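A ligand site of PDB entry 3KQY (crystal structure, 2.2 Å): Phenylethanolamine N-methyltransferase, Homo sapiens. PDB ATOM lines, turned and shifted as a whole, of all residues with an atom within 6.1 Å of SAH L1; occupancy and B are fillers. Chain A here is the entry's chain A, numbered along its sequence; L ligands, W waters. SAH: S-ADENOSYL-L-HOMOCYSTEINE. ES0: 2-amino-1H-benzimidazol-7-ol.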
ATOM      1  N   TYR A  27       6.642  29.791   6.082  1.00  0.00           N
ATOM      2  CA  TYR A  27       7.405  28.719   5.447  1.00  0.00           C
ATOM      3  C   TYR A  27       8.455  28.112   6.369  1.00  0.00           C
ATOM      4  O   TYR A  27       9.102  27.131   6.024  1.00  0.00           O
ATOM      5  CB  TYR A  27       8.042  29.197   4.143  1.00  0.00           C
ATOM      6  CG  TYR A  27       7.104  29.081   2.954  1.00  0.00           C
ATOM      7  CD1 TYR A  27       6.489  30.206   2.423  1.00  0.00           C
ATOM      8  CD2 TYR A  27       6.832  27.845   2.390  1.00  0.00           C
ATOM      9  CE1 TYR A  27       5.622  30.100   1.350  1.00  0.00           C
ATOM     10  CE2 TYR A  27       5.966  27.729   1.313  1.00  0.00           C
ATOM     11  CZ  TYR A  27       5.371  28.862   0.794  1.00  0.00           C
ATOM     12  OH  TYR A  27       4.505  28.743  -0.273  1.00  0.00           O
ATOM     13  N   PHE A  30       6.996  24.835   7.361  1.00  0.00           N
ATOM     14  CA  PHE A  30       6.797  23.935   6.226  1.00  0.00           C
ATOM     15  C   PHE A  30       7.442  22.552   6.430  1.00  0.00           C
ATOM     16  O   PHE A  30       8.667  22.441   6.525  1.00  0.00           O
ATOM     17  CB  PHE A  30       7.360  24.615   4.974  1.00  0.00           C
ATOM     18  CG  PHE A  30       7.095  23.882   3.691  1.00  0.00           C
ATOM     19  CD1 PHE A  30       6.061  24.265   2.859  1.00  0.00           C
ATOM     20  CD2 PHE A  30       7.922  22.836   3.292  1.00  0.00           C
ATOM     21  CE1 PHE A  30       5.825  23.599   1.669  1.00  0.00           C
ATOM     22  CE2 PHE A  30       7.696  22.180   2.104  1.00  0.00           C
ATOM     23  CZ  PHE A  30       6.642  22.569   1.284  1.00  0.00           C
ATOM     24  N   TYR A  35       4.020  17.749   2.988  1.00  0.00           N
ATOM     25  CA  TYR A  35       3.694  18.343   1.690  1.00  0.00           C
ATOM     26  C   TYR A  35       3.659  17.278   0.596  1.00  0.00           C
ATOM     27  O   TYR A  35       2.717  17.211  -0.193  1.00  0.00           O
ATOM     28  CB  TYR A  35       4.694  19.443   1.342  1.00  0.00           C
ATOM     29  CG  TYR A  35       4.536  20.016  -0.050  1.00  0.00           C
ATOM     30  CD1 TYR A  35       3.471  20.860  -0.361  1.00  0.00           C
ATOM     31  CD2 TYR A  35       5.447  19.700  -1.050  1.00  0.00           C
ATOM     32  CE1 TYR A  35       3.328  21.377  -1.634  1.00  0.00           C
ATOM     33  CE2 TYR A  35       5.303  20.217  -2.323  1.00  0.00           C
ATOM     34  CZ  TYR A  35       4.248  21.046  -2.618  1.00  0.00           C
ATOM     35  OH  TYR A  35       4.105  21.551  -3.884  1.00  0.00           O
ATOM     36  N   TYR A  40       1.424  14.385  -3.461  1.00  0.00           N
ATOM     37  CA  TYR A  40       2.081  13.426  -4.342  1.00  0.00           C
ATOM     38  C   TYR A  40       1.961  11.974  -3.879  1.00  0.00           C
ATOM     39  O   TYR A  40       2.633  11.088  -4.406  1.00  0.00           O
ATOM     40  CB  TYR A  40       3.538  13.829  -4.562  1.00  0.00           C
ATOM     41  CG  TYR A  40       3.617  15.214  -5.158  1.00  0.00           C
ATOM     42  CD1 TYR A  40       3.905  16.320  -4.361  1.00  0.00           C
ATOM     43  CD2 TYR A  40       3.348  15.426  -6.497  1.00  0.00           C
ATOM     44  CE1 TYR A  40       3.957  17.583  -4.898  1.00  0.00           C
ATOM     45  CE2 TYR A  40       3.400  16.692  -7.044  1.00  0.00           C
ATOM     46  CZ  TYR A  40       3.700  17.763  -6.236  1.00  0.00           C
ATOM     47  OH  TYR A  40       3.752  19.020  -6.786  1.00  0.00           O
ATOM     48  N   LYS A  57      -0.354  16.861 -15.650  1.00  0.00           N
ATOM     49  CA  LYS A  57       0.860  17.658 -15.560  1.00  0.00           C
ATOM     50  C   LYS A  57       2.010  17.073 -16.374  1.00  0.00           C
ATOM     51  O   LYS A  57       2.640  17.768 -17.176  1.00  0.00           O
ATOM     52  CB  LYS A  57       1.312  17.813 -14.108  1.00  0.00           C
ATOM     53  CG  LYS A  57       0.415  18.733 -13.284  1.00  0.00           C
ATOM     54  CD  LYS A  57       1.042  19.027 -11.941  1.00  0.00           C
ATOM     55  CE  LYS A  57       0.935  17.837 -11.017  1.00  0.00           C
ATOM     56  NZ  LYS A  57       1.571  18.133  -9.715  1.00  0.00           N
ATOM     57  N   ASP A  77      15.406  25.050 -12.208  1.00  0.00           N
ATOM     58  CA  ASP A  77      14.102  24.794 -11.626  1.00  0.00           C
ATOM     59  C   ASP A  77      13.910  25.747 -10.446  1.00  0.00           C
ATOM     60  O   ASP A  77      14.640  25.657  -9.458  1.00  0.00           O
ATOM     61  CB  ASP A  77      14.003  23.337 -11.144  1.00  0.00           C
ATOM     62  CG  ASP A  77      12.619  22.974 -10.665  1.00  0.00           C
ATOM     63  OD1 ASP A  77      11.637  23.451 -11.284  1.00  0.00           O
ATOM     64  OD2 ASP A  77      12.503  22.222  -9.674  1.00  0.00           O
ATOM     65  N   ILE A  78      12.918  26.635 -10.547  1.00  0.00           N
ATOM     66  CA  ILE A  78      12.672  27.659  -9.543  1.00  0.00           C
ATOM     67  C   ILE A  78      11.732  27.176  -8.452  1.00  0.00           C
ATOM     68  O   ILE A  78      10.553  26.908  -8.711  1.00  0.00           O
ATOM     69  CB  ILE A  78      12.023  28.906 -10.172  1.00  0.00           C
ATOM     70  CG1 ILE A  78      12.841  29.407 -11.369  1.00  0.00           C
ATOM     71  CG2 ILE A  78      11.836  29.993  -9.130  1.00  0.00           C
ATOM     72  CD1 ILE A  78      14.302  29.620 -11.081  1.00  0.00           C
ATOM     73  N   GLY A  79      12.225  27.096  -7.226  1.00  0.00           N
ATOM     74  CA  GLY A  79      11.393  26.689  -6.106  1.00  0.00           C
ATOM     75  C   GLY A  79      10.994  25.226  -6.223  1.00  0.00           C
ATOM     76  O   GLY A  79       9.812  24.894  -6.157  1.00  0.00           O
ATOM     77  N   SER A  80      12.001  24.376  -6.393  1.00  0.00           N
ATOM     78  CA  SER A  80      11.800  22.944  -6.568  1.00  0.00           C
ATOM     79  C   SER A  80      11.014  22.305  -5.434  1.00  0.00           C
ATOM     80  O   SER A  80      10.231  21.377  -5.656  1.00  0.00           O
ATOM     81  CB  SER A  80      13.155  22.241  -6.682  1.00  0.00           C
ATOM     82  OG  SER A  80      13.925  22.755  -7.748  1.00  0.00           O
ATOM     83  N   GLY A  81      11.234  22.794  -4.211  1.00  0.00           N
ATOM     84  CA  GLY A  81      10.689  22.128  -3.039  1.00  0.00           C
ATOM     85  C   GLY A  81      11.353  20.775  -2.899  1.00  0.00           C
ATOM     86  O   GLY A  81      12.531  20.617  -3.213  1.00  0.00           O
ATOM     87  N   PRO A  82      10.593  19.763  -2.448  1.00  0.00           N
ATOM     88  CA  PRO A  82      11.126  18.410  -2.315  1.00  0.00           C
ATOM     89  C   PRO A  82      10.685  17.557  -3.483  1.00  0.00           C
ATOM     90  O   PRO A  82      10.556  16.348  -3.313  1.00  0.00           O
ATOM     91  CB  PRO A  82      10.420  17.892  -1.054  1.00  0.00           C
ATOM     92  CG  PRO A  82       9.181  18.799  -0.883  1.00  0.00           C
ATOM     93  CD  PRO A  82       9.189  19.814  -1.993  1.00  0.00           C
ATOM     94  N   THR A  83      10.421  18.154  -4.646  1.00  0.00           N
ATOM     95  CA  THR A  83       9.880  17.377  -5.758  1.00  0.00           C
ATOM     96  C   THR A  83      10.779  17.369  -6.991  1.00  0.00           C
ATOM     97  O   THR A  83      11.585  18.279  -7.202  1.00  0.00           O
ATOM     98  CB  THR A  83       8.443  17.798  -6.142  1.00  0.00           C
ATOM     99  OG1 THR A  83       8.462  19.001  -6.936  1.00  0.00           O
ATOM    100  CG2 THR A  83       7.589  18.003  -4.904  1.00  0.00           C
ATOM    101  N   TYR A  85       9.417  15.478 -10.108  1.00  0.00           N
ATOM    102  CA  TYR A  85       8.585  15.123 -11.256  1.00  0.00           C
ATOM    103  C   TYR A  85       8.672  16.174 -12.346  1.00  0.00           C
ATOM    104  O   TYR A  85       8.629  15.846 -13.536  1.00  0.00           O
ATOM    105  CB  TYR A  85       7.126  14.962 -10.830  1.00  0.00           C
ATOM    106  CG  TYR A  85       6.461  16.277 -10.522  1.00  0.00           C
ATOM    107  CD1 TYR A  85       5.768  16.979 -11.498  1.00  0.00           C
ATOM    108  CD2 TYR A  85       6.540  16.844  -9.253  1.00  0.00           C
ATOM    109  CE1 TYR A  85       5.165  18.190 -11.223  1.00  0.00           C
ATOM    110  CE2 TYR A  85       5.947  18.053  -8.968  1.00  0.00           C
ATOM    111  CZ  TYR A  85       5.265  18.716  -9.955  1.00  0.00           C
ATOM    112  OH  TYR A  85       4.672  19.928  -9.680  1.00  0.00           O
ATOM    113  N   GLN A  86       8.801  17.445 -11.945  1.00  0.00           N
ATOM    114  CA  GLN A  86       8.779  18.556 -12.891  1.00  0.00           C
ATOM    115  C   GLN A  86       9.953  18.549 -13.859  1.00  0.00           C
ATOM    116  O   GLN A  86       9.930  19.243 -14.875  1.00  0.00           O
ATOM    117  CB  GLN A  86       8.671  19.913 -12.156  1.00  0.00           C
ATOM    118  CG  GLN A  86       9.878  20.280 -11.275  1.00  0.00           C
ATOM    119  CD  GLN A  86       9.755  19.758  -9.862  1.00  0.00           C
ATOM    120  OE1 GLN A  86       8.980  18.844  -9.600  1.00  0.00           O
ATOM    121  NE2 GLN A  86      10.518  20.335  -8.939  1.00  0.00           N
ATOM    122  N   ASP A 101      15.621  25.869  -3.946  1.00  0.00           N
ATOM    123  CA  ASP A 101      14.519  26.158  -3.043  1.00  0.00           C
ATOM    124  C   ASP A 101      14.919  27.069  -1.899  1.00  0.00           C
ATOM    125  O   ASP A 101      16.067  27.081  -1.444  1.00  0.00           O
ATOM    126  CB  ASP A 101      13.867  24.899  -2.490  1.00  0.00           C
ATOM    127  CG  ASP A 101      12.449  25.166  -1.992  1.00  0.00           C
ATOM    128  OD1 ASP A 101      11.588  25.461  -2.833  1.00  0.00           O
ATOM    129  OD2 ASP A 101      12.222  25.084  -0.770  1.00  0.00           O
ATOM    130  N   PHE A 102      13.939  27.829  -1.423  1.00  0.00           N
ATOM    131  CA  PHE A 102      14.146  28.791  -0.354  1.00  0.00           C
ATOM    132  C   PHE A 102      14.485  28.086   0.963  1.00  0.00           C
ATOM    133  O   PHE A 102      15.287  28.592   1.739  1.00  0.00           O
ATOM    134  CB  PHE A 102      12.888  29.662  -0.204  1.00  0.00           C
ATOM    135  CG  PHE A 102      12.975  30.663   0.901  1.00  0.00           C
ATOM    136  CD1 PHE A 102      13.737  31.812   0.761  1.00  0.00           C
ATOM    137  CD2 PHE A 102      12.259  30.474   2.071  1.00  0.00           C
ATOM    138  CE1 PHE A 102      13.803  32.743   1.783  1.00  0.00           C
ATOM    139  CE2 PHE A 102      12.316  31.395   3.091  1.00  0.00           C
ATOM    140  CZ  PHE A 102      13.088  32.534   2.948  1.00  0.00           C
ATOM    141  N   LEU A 103      13.905  26.907   1.184  1.00  0.00           N
ATOM    142  CA  LEU A 103      14.093  26.187   2.438  1.00  0.00           C
ATOM    143  C   LEU A 103      15.227  25.162   2.412  1.00  0.00           C
ATOM    144  O   LEU A 103      15.358  24.387   1.473  1.00  0.00           O
ATOM    145  CB  LEU A 103      12.806  25.505   2.873  1.00  0.00           C
ATOM    146  CG  LEU A 103      11.640  26.432   3.194  1.00  0.00           C
ATOM    147  CD1 LEU A 103      10.372  25.641   3.472  1.00  0.00           C
ATOM    148  CD2 LEU A 103      12.000  27.332   4.377  1.00  0.00           C
ATOM    149  N   ASN A 106      13.969  21.465   2.359  1.00  0.00           N
ATOM    150  CA  ASN A 106      13.618  20.950   1.039  1.00  0.00           C
ATOM    151  C   ASN A 106      14.853  20.558   0.248  1.00  0.00           C
ATOM    152  O   ASN A 106      14.854  19.555  -0.453  1.00  0.00           O
ATOM    153  CB  ASN A 106      12.801  21.970   0.252  1.00  0.00           C
ATOM    154  CG  ASN A 106      11.347  21.946   0.635  1.00  0.00           C
ATOM    155  OD1 ASN A 106      10.611  22.921   0.396  1.00  0.00           O
ATOM    156  ND2 ASN A 106      10.902  20.846   1.229  1.00  0.00           N
ATOM    157  N   ILE A 157      17.416  29.966  -2.954  1.00  0.00           N
ATOM    158  CA  ILE A 157      16.857  30.978  -3.843  1.00  0.00           C
ATOM    159  C   ILE A 157      15.761  31.760  -3.128  1.00  0.00           C
ATOM    160  O   ILE A 157      15.088  31.236  -2.234  1.00  0.00           O
ATOM    161  CB  ILE A 157      16.300  30.314  -5.129  1.00  0.00           C
ATOM    162  CG1 ILE A 157      15.898  31.372  -6.164  1.00  0.00           C
ATOM    163  CG2 ILE A 157      15.136  29.394  -4.798  1.00  0.00           C
ATOM    164  CD1 ILE A 157      15.478  30.789  -7.503  1.00  0.00           C
ATOM    165  N   ASP A 158      15.606  33.032  -3.492  1.00  0.00           N
ATOM    166  CA  ASP A 158      14.505  33.875  -3.020  1.00  0.00           C
ATOM    167  C   ASP A 158      14.006  34.701  -4.194  1.00  0.00           C
ATOM    168  O   ASP A 158      14.667  35.641  -4.622  1.00  0.00           O
ATOM    169  CB  ASP A 158      14.953  34.803  -1.894  1.00  0.00           C
ATOM    170  CG  ASP A 158      13.795  35.607  -1.296  1.00  0.00           C
ATOM    171  OD1 ASP A 158      12.731  35.705  -1.941  1.00  0.00           O
ATOM    172  OD2 ASP A 158      13.962  36.148  -0.183  1.00  0.00           O
ATOM    173  N   VAL A 159      12.824  34.351  -4.706  1.00  0.00           N
ATOM    174  CA  VAL A 159      12.298  35.021  -5.883  1.00  0.00           C
ATOM    175  C   VAL A 159      11.931  36.470  -5.585  1.00  0.00           C
ATOM    176  O   VAL A 159      11.717  37.264  -6.494  1.00  0.00           O
ATOM    177  CB  VAL A 159      11.075  34.276  -6.437  1.00  0.00           C
ATOM    178  CG1 VAL A 159      11.487  32.912  -6.952  1.00  0.00           C
ATOM    179  CG2 VAL A 159      10.016  34.151  -5.365  1.00  0.00           C
ATOM    180  N   HIS A 160      11.885  36.809  -4.296  1.00  0.00           N
ATOM    181  CA  HIS A 160      11.552  38.159  -3.871  1.00  0.00           C
ATOM    182  C   HIS A 160      12.727  39.113  -4.068  1.00  0.00           C
ATOM    183  O   HIS A 160      12.560  40.328  -4.062  1.00  0.00           O
ATOM    184  CB  HIS A 160      11.087  38.162  -2.421  1.00  0.00           C
ATOM    185  CG  HIS A 160       9.775  37.475  -2.216  1.00  0.00           C
ATOM    186  ND1 HIS A 160       8.747  37.550  -3.138  1.00  0.00           N
ATOM    187  CD2 HIS A 160       9.310  36.719  -1.196  1.00  0.00           C
ATOM    188  CE1 HIS A 160       7.710  36.861  -2.701  1.00  0.00           C
ATOM    189  NE2 HIS A 160       8.022  36.344  -1.525  1.00  0.00           N
ATOM    190  N   SER A 180       9.217  26.239 -13.327  1.00  0.00           N
ATOM    191  CA  SER A 180       8.736  26.457 -11.969  1.00  0.00           C
ATOM    192  C   SER A 180       7.320  25.944 -11.762  1.00  0.00           C
ATOM    193  O   SER A 180       6.419  26.246 -12.559  1.00  0.00           O
ATOM    194  CB  SER A 180       8.809  27.939 -11.578  1.00  0.00           C
ATOM    195  OG  SER A 180       8.408  28.108 -10.226  1.00  0.00           O
ATOM    196  N   ALA A 181       7.126  25.206 -10.681  1.00  0.00           N
ATOM    197  CA  ALA A 181       5.803  24.667 -10.380  1.00  0.00           C
ATOM    198  C   ALA A 181       5.329  24.995  -8.970  1.00  0.00           C
ATOM    199  O   ALA A 181       6.004  24.686  -7.982  1.00  0.00           O
ATOM    200  CB  ALA A 181       5.773  23.154 -10.625  1.00  0.00           C
ATOM    201  N   PHE A 182       4.156  25.629  -8.891  1.00  0.00           N
ATOM    202  CA  PHE A 182       3.511  25.932  -7.620  1.00  0.00           C
ATOM    203  C   PHE A 182       4.368  26.796  -6.678  1.00  0.00           C
ATOM    204  O   PHE A 182       4.241  26.707  -5.460  1.00  0.00           O
ATOM    205  CB  PHE A 182       3.093  24.631  -6.907  1.00  0.00           C
ATOM    206  CG  PHE A 182       2.178  23.770  -7.721  1.00  0.00           C
ATOM    207  CD1 PHE A 182       2.643  22.616  -8.342  1.00  0.00           C
ATOM    208  CD2 PHE A 182       0.837  24.114  -7.870  1.00  0.00           C
ATOM    209  CE1 PHE A 182       1.788  21.819  -9.087  1.00  0.00           C
ATOM    210  CE2 PHE A 182      -0.018  23.317  -8.615  1.00  0.00           C
ATOM    211  CZ  PHE A 182       0.457  22.169  -9.223  1.00  0.00           C
ATOM    212  N   CYS A 183       5.219  27.637  -7.254  1.00  0.00           N
ATOM    213  CA  CYS A 183       6.044  28.515  -6.433  1.00  0.00           C
ATOM    214  C   CYS A 183       5.454  29.927  -6.307  1.00  0.00           C
ATOM    215  O   CYS A 183       4.933  30.291  -5.270  1.00  0.00           O
ATOM    216  CB  CYS A 183       7.473  28.615  -6.969  1.00  0.00           C
ATOM    217  SG  CYS A 183       8.592  29.498  -5.862  1.00  0.00           S
ATOM    218  N   ALA A 186       2.440  30.840  -4.695  1.00  0.00           N
ATOM    219  CA  ALA A 186       2.476  30.288  -3.346  1.00  0.00           C
ATOM    220  C   ALA A 186       3.355  31.090  -2.371  1.00  0.00           C
ATOM    221  O   ALA A 186       3.331  30.842  -1.172  1.00  0.00           O
ATOM    222  CB  ALA A 186       2.928  28.835  -3.377  1.00  0.00           C
ATOM    223  N   VAL A 187       4.124  32.032  -2.905  1.00  0.00           N
ATOM    224  CA  VAL A 187       5.000  32.858  -2.080  1.00  0.00           C
ATOM    225  C   VAL A 187       4.683  34.351  -2.249  1.00  0.00           C
ATOM    226  O   VAL A 187       5.393  35.215  -1.742  1.00  0.00           O
ATOM    227  CB  VAL A 187       6.491  32.615  -2.406  1.00  0.00           C
ATOM    228  CG1 VAL A 187       6.806  31.128  -2.328  1.00  0.00           C
ATOM    229  CG2 VAL A 187       6.835  33.159  -3.776  1.00  0.00           C
ATOM    230  N   TYR A 222      -2.858  26.470   1.416  1.00  0.00           N
ATOM    231  CA  TYR A 222      -2.585  25.050   1.441  1.00  0.00           C
ATOM    232  C   TYR A 222      -1.765  24.712   2.677  1.00  0.00           C
ATOM    233  O   TYR A 222      -0.975  25.526   3.147  1.00  0.00           O
ATOM    234  CB  TYR A 222      -1.866  24.603   0.167  1.00  0.00           C
ATOM    235  CG  TYR A 222      -0.416  24.983   0.097  1.00  0.00           C
ATOM    236  CD1 TYR A 222       0.572  24.093   0.522  1.00  0.00           C
ATOM    237  CD2 TYR A 222      -0.012  26.209  -0.397  1.00  0.00           C
ATOM    238  CE1 TYR A 222       1.904  24.426   0.462  1.00  0.00           C
ATOM    239  CE2 TYR A 222       1.330  26.554  -0.463  1.00  0.00           C
ATOM    240  CZ  TYR A 222       2.278  25.661  -0.029  1.00  0.00           C
ATOM    241  OH  TYR A 222       3.610  25.984  -0.091  1.00  0.00           O
HETATM  242  N   SAH L   1       7.911  22.930  -7.000  1.00  0.00           N
HETATM  243  CA  SAH L   1       7.410  21.985  -6.015  1.00  0.00           C
HETATM  244  CB  SAH L   1       7.187  22.683  -4.679  1.00  0.00           C
HETATM  245  CG  SAH L   1       6.189  23.834  -4.786  1.00  0.00           C
HETATM  246  SD  SAH L   1       5.624  24.386  -3.151  1.00  0.00           S
HETATM  247  C   SAH L   1       6.135  21.332  -6.530  1.00  0.00           C
HETATM  248  O   SAH L   1       5.523  20.668  -5.761  1.00  0.00           O
HETATM  249  OXT SAH L   1       5.878  21.479  -7.898  1.00  0.00           O
HETATM  250  C5' SAH L   1       6.338  26.051  -3.066  1.00  0.00           C
HETATM  251  C4' SAH L   1       7.832  26.154  -2.759  1.00  0.00           C
HETATM  252  O4' SAH L   1       8.232  27.474  -2.756  1.00  0.00           O
HETATM  253  C3' SAH L   1       8.228  25.608  -1.407  1.00  0.00           C
HETATM  254  O3' SAH L   1       9.197  24.601  -1.610  1.00  0.00           O
HETATM  255  C2' SAH L   1       8.774  26.698  -0.756  1.00  0.00           C
HETATM  256  O2' SAH L   1       9.798  26.378   0.147  1.00  0.00           O
HETATM  257  C1' SAH L   1       9.237  27.547  -1.810  1.00  0.00           C
HETATM  258  N9  SAH L   1       9.493  28.923  -1.403  1.00  0.00           N
HETATM  259  C8  SAH L   1       9.028  29.518  -0.299  1.00  0.00           C
HETATM  260  N7  SAH L   1       9.469  30.832  -0.310  1.00  0.00           N
HETATM  261  C5  SAH L   1      10.195  31.033  -1.447  1.00  0.00           C
HETATM  262  C6  SAH L   1      10.842  32.126  -1.934  1.00  0.00           C
HETATM  263  N6  SAH L   1      10.806  33.379  -1.201  1.00  0.00           N
HETATM  264  N1  SAH L   1      11.493  32.061  -3.094  1.00  0.00           N
HETATM  265  C2  SAH L   1      11.518  30.885  -3.774  1.00  0.00           C
HETATM  266  N3  SAH L   1      10.881  29.793  -3.286  1.00  0.00           N
HETATM  267  C4  SAH L   1      10.219  29.876  -2.120  1.00  0.00           C
HETATM  268  NAA ES0 L   2       1.562  22.459  -4.537  1.00  0.00           N
HETATM  269  OAB ES0 L   2      -3.372  21.310  -6.173  1.00  0.00           O
HETATM  270  CAC ES0 L   2      -1.441  18.703  -7.828  1.00  0.00           C
HETATM  271  CAD ES0 L   2      -2.522  19.481  -7.418  1.00  0.00           C
HETATM  272  CAE ES0 L   2      -0.160  19.015  -7.392  1.00  0.00           C
HETATM  273  NAF ES0 L   2       1.129  20.622  -5.972  1.00  0.00           N
HETATM  274  NAG ES0 L   2      -0.568  21.826  -5.349  1.00  0.00           N
HETATM  275  CAH ES0 L   2       0.747  21.674  -5.248  1.00  0.00           C
HETATM  276  CAI ES0 L   2      -2.322  20.561  -6.574  1.00  0.00           C
HETATM  277  CAJ ES0 L   2       0.040  20.101  -6.536  1.00  0.00           C
HETATM  278  CAK ES0 L   2      -1.041  20.872  -6.139  1.00  0.00           C
HETATM  279  O   HOH W   1       9.802  23.882  -9.206  1.00  0.00           O
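The backbone carbonyl oxygen (O) of Phe 182 sits close to a sulfur (SD) of SAH L1, at 3.6 Å.
Tyr 27 touches SAH L1 (CE2 to C2', 3.6 Å).
Gly 81 touches SAH L1.
OG1 of Thr 83 touches CA of SAH L1 (3.3 Å).
Phe 102 touches SAH L1 (CB to C5, 3.3 Å).
CD1 of Leu 103 touches O2' of SAH L1, at 3.5 Å.
Ile 157 touches SAH L1 (O to N1, 3.8 Å).
His 160 touches SAH L1 (CD2 to N6, 3.7 Å).
CG1 of Val 187 touches N7 of SAH L1 (3.4 Å).
Tyr 222 touches SAH L1 (OH to SD, 3.997 Å).
21 residues have an atom within 4 Å of SAH L1: Tyr 27, Tyr 35, Tyr 40, Gly 79, Ser 80, Gly 81, Thr 83, Tyr 85, Asp 101, Phe 102, Leu 103, Asn 106, Ile 157, Asp 158, Val 159, His 160, Ala 181, Phe 182, Cys 183, Val 187 and Tyr 222.
The nearest printed residue that does not touch SAH L1 is Gln 86 (4.2 Å).
The side-chain hydroxyl (OH) of Tyr 85 is in hydrogen-bond range of the side-chain hydroxyl (OH) of Tyr 40, at 3.2 Å.
OD1 of Asn 106 lies close to OD2 of Asp 101 (2.9 Å).
The side-chain carboxylate (OD1) of Asp 101 is in hydrogen-bond range of the backbone NH (N) of Gly 81 (3.0 Å).
N of Leu 103 is in hydrogen-bond range of OD2 of Asp 101 (3.2 Å).
The backbone carbonyl oxygen of Ser 80 lies within hydrogen-bond range of the side-chain hydroxyl of Thr 83 (3.2 Å).
The backbone carbonyl oxygen of Ser 80 sits at hydrogen-bond distance from the side-chain amide nitrogen of Gln 86.
The side-chain carboxylate of Asp 77 lies within hydrogen-bond range of the side-chain hydroxyl of Ser 80.
NE2 of His 160 lies within hydrogen-bond range of O of Val 187, 2.9 Å away.
An oxygen (O) of SAH L1 sits at hydrogen-bond distance from the side-chain hydroxyl of Tyr 35 (2.5 Å).
OH of Tyr 40 lies within hydrogen-bond range of O of SAH L1 (2.6 Å).
An oxygen (OXT) of SAH L1 lies within hydrogen-bond range of the side-chain hydroxyl of Tyr 85.
O of Ala 181 lies within hydrogen-bond range of N of SAH L1.
O3' of SAH L1 is in hydrogen-bond range of OD1 of Asp 101, 2.8 Å away.
O of Gly 79 sits at hydrogen-bond distance from N of SAH L1, 2.9 Å away.
A nitrogen (N) of SAH L1 lies close to the backbone carbonyl oxygen of Ser 80, at 3.1 Å.
The side-chain amide oxygen of Asn 106 is in hydrogen-bond range of an oxygen (O3') of SAH L1 (3.0 Å).
N1 of SAH L1 lies within hydrogen-bond range of N of Val 159 (3.1 Å).
OD1 of Asp 158 sits at hydrogen-bond distance from N6 of SAH L1, 3.1 Å away.
SG of Cys 183 is in hydrogen-bond range of N3 of SAH L1 (3.5 Å).
The side-chain hydroxyl (OH) of Tyr 35 is in hydrogen-bond range of a nitrogen (NAA) of ES0 L2, 2.8 Å away.
A nitrogen (NAF) of ES0 L2 sits at hydrogen-bond distance from the side-chain hydroxyl (OH) of Tyr 40 (3.2 Å).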
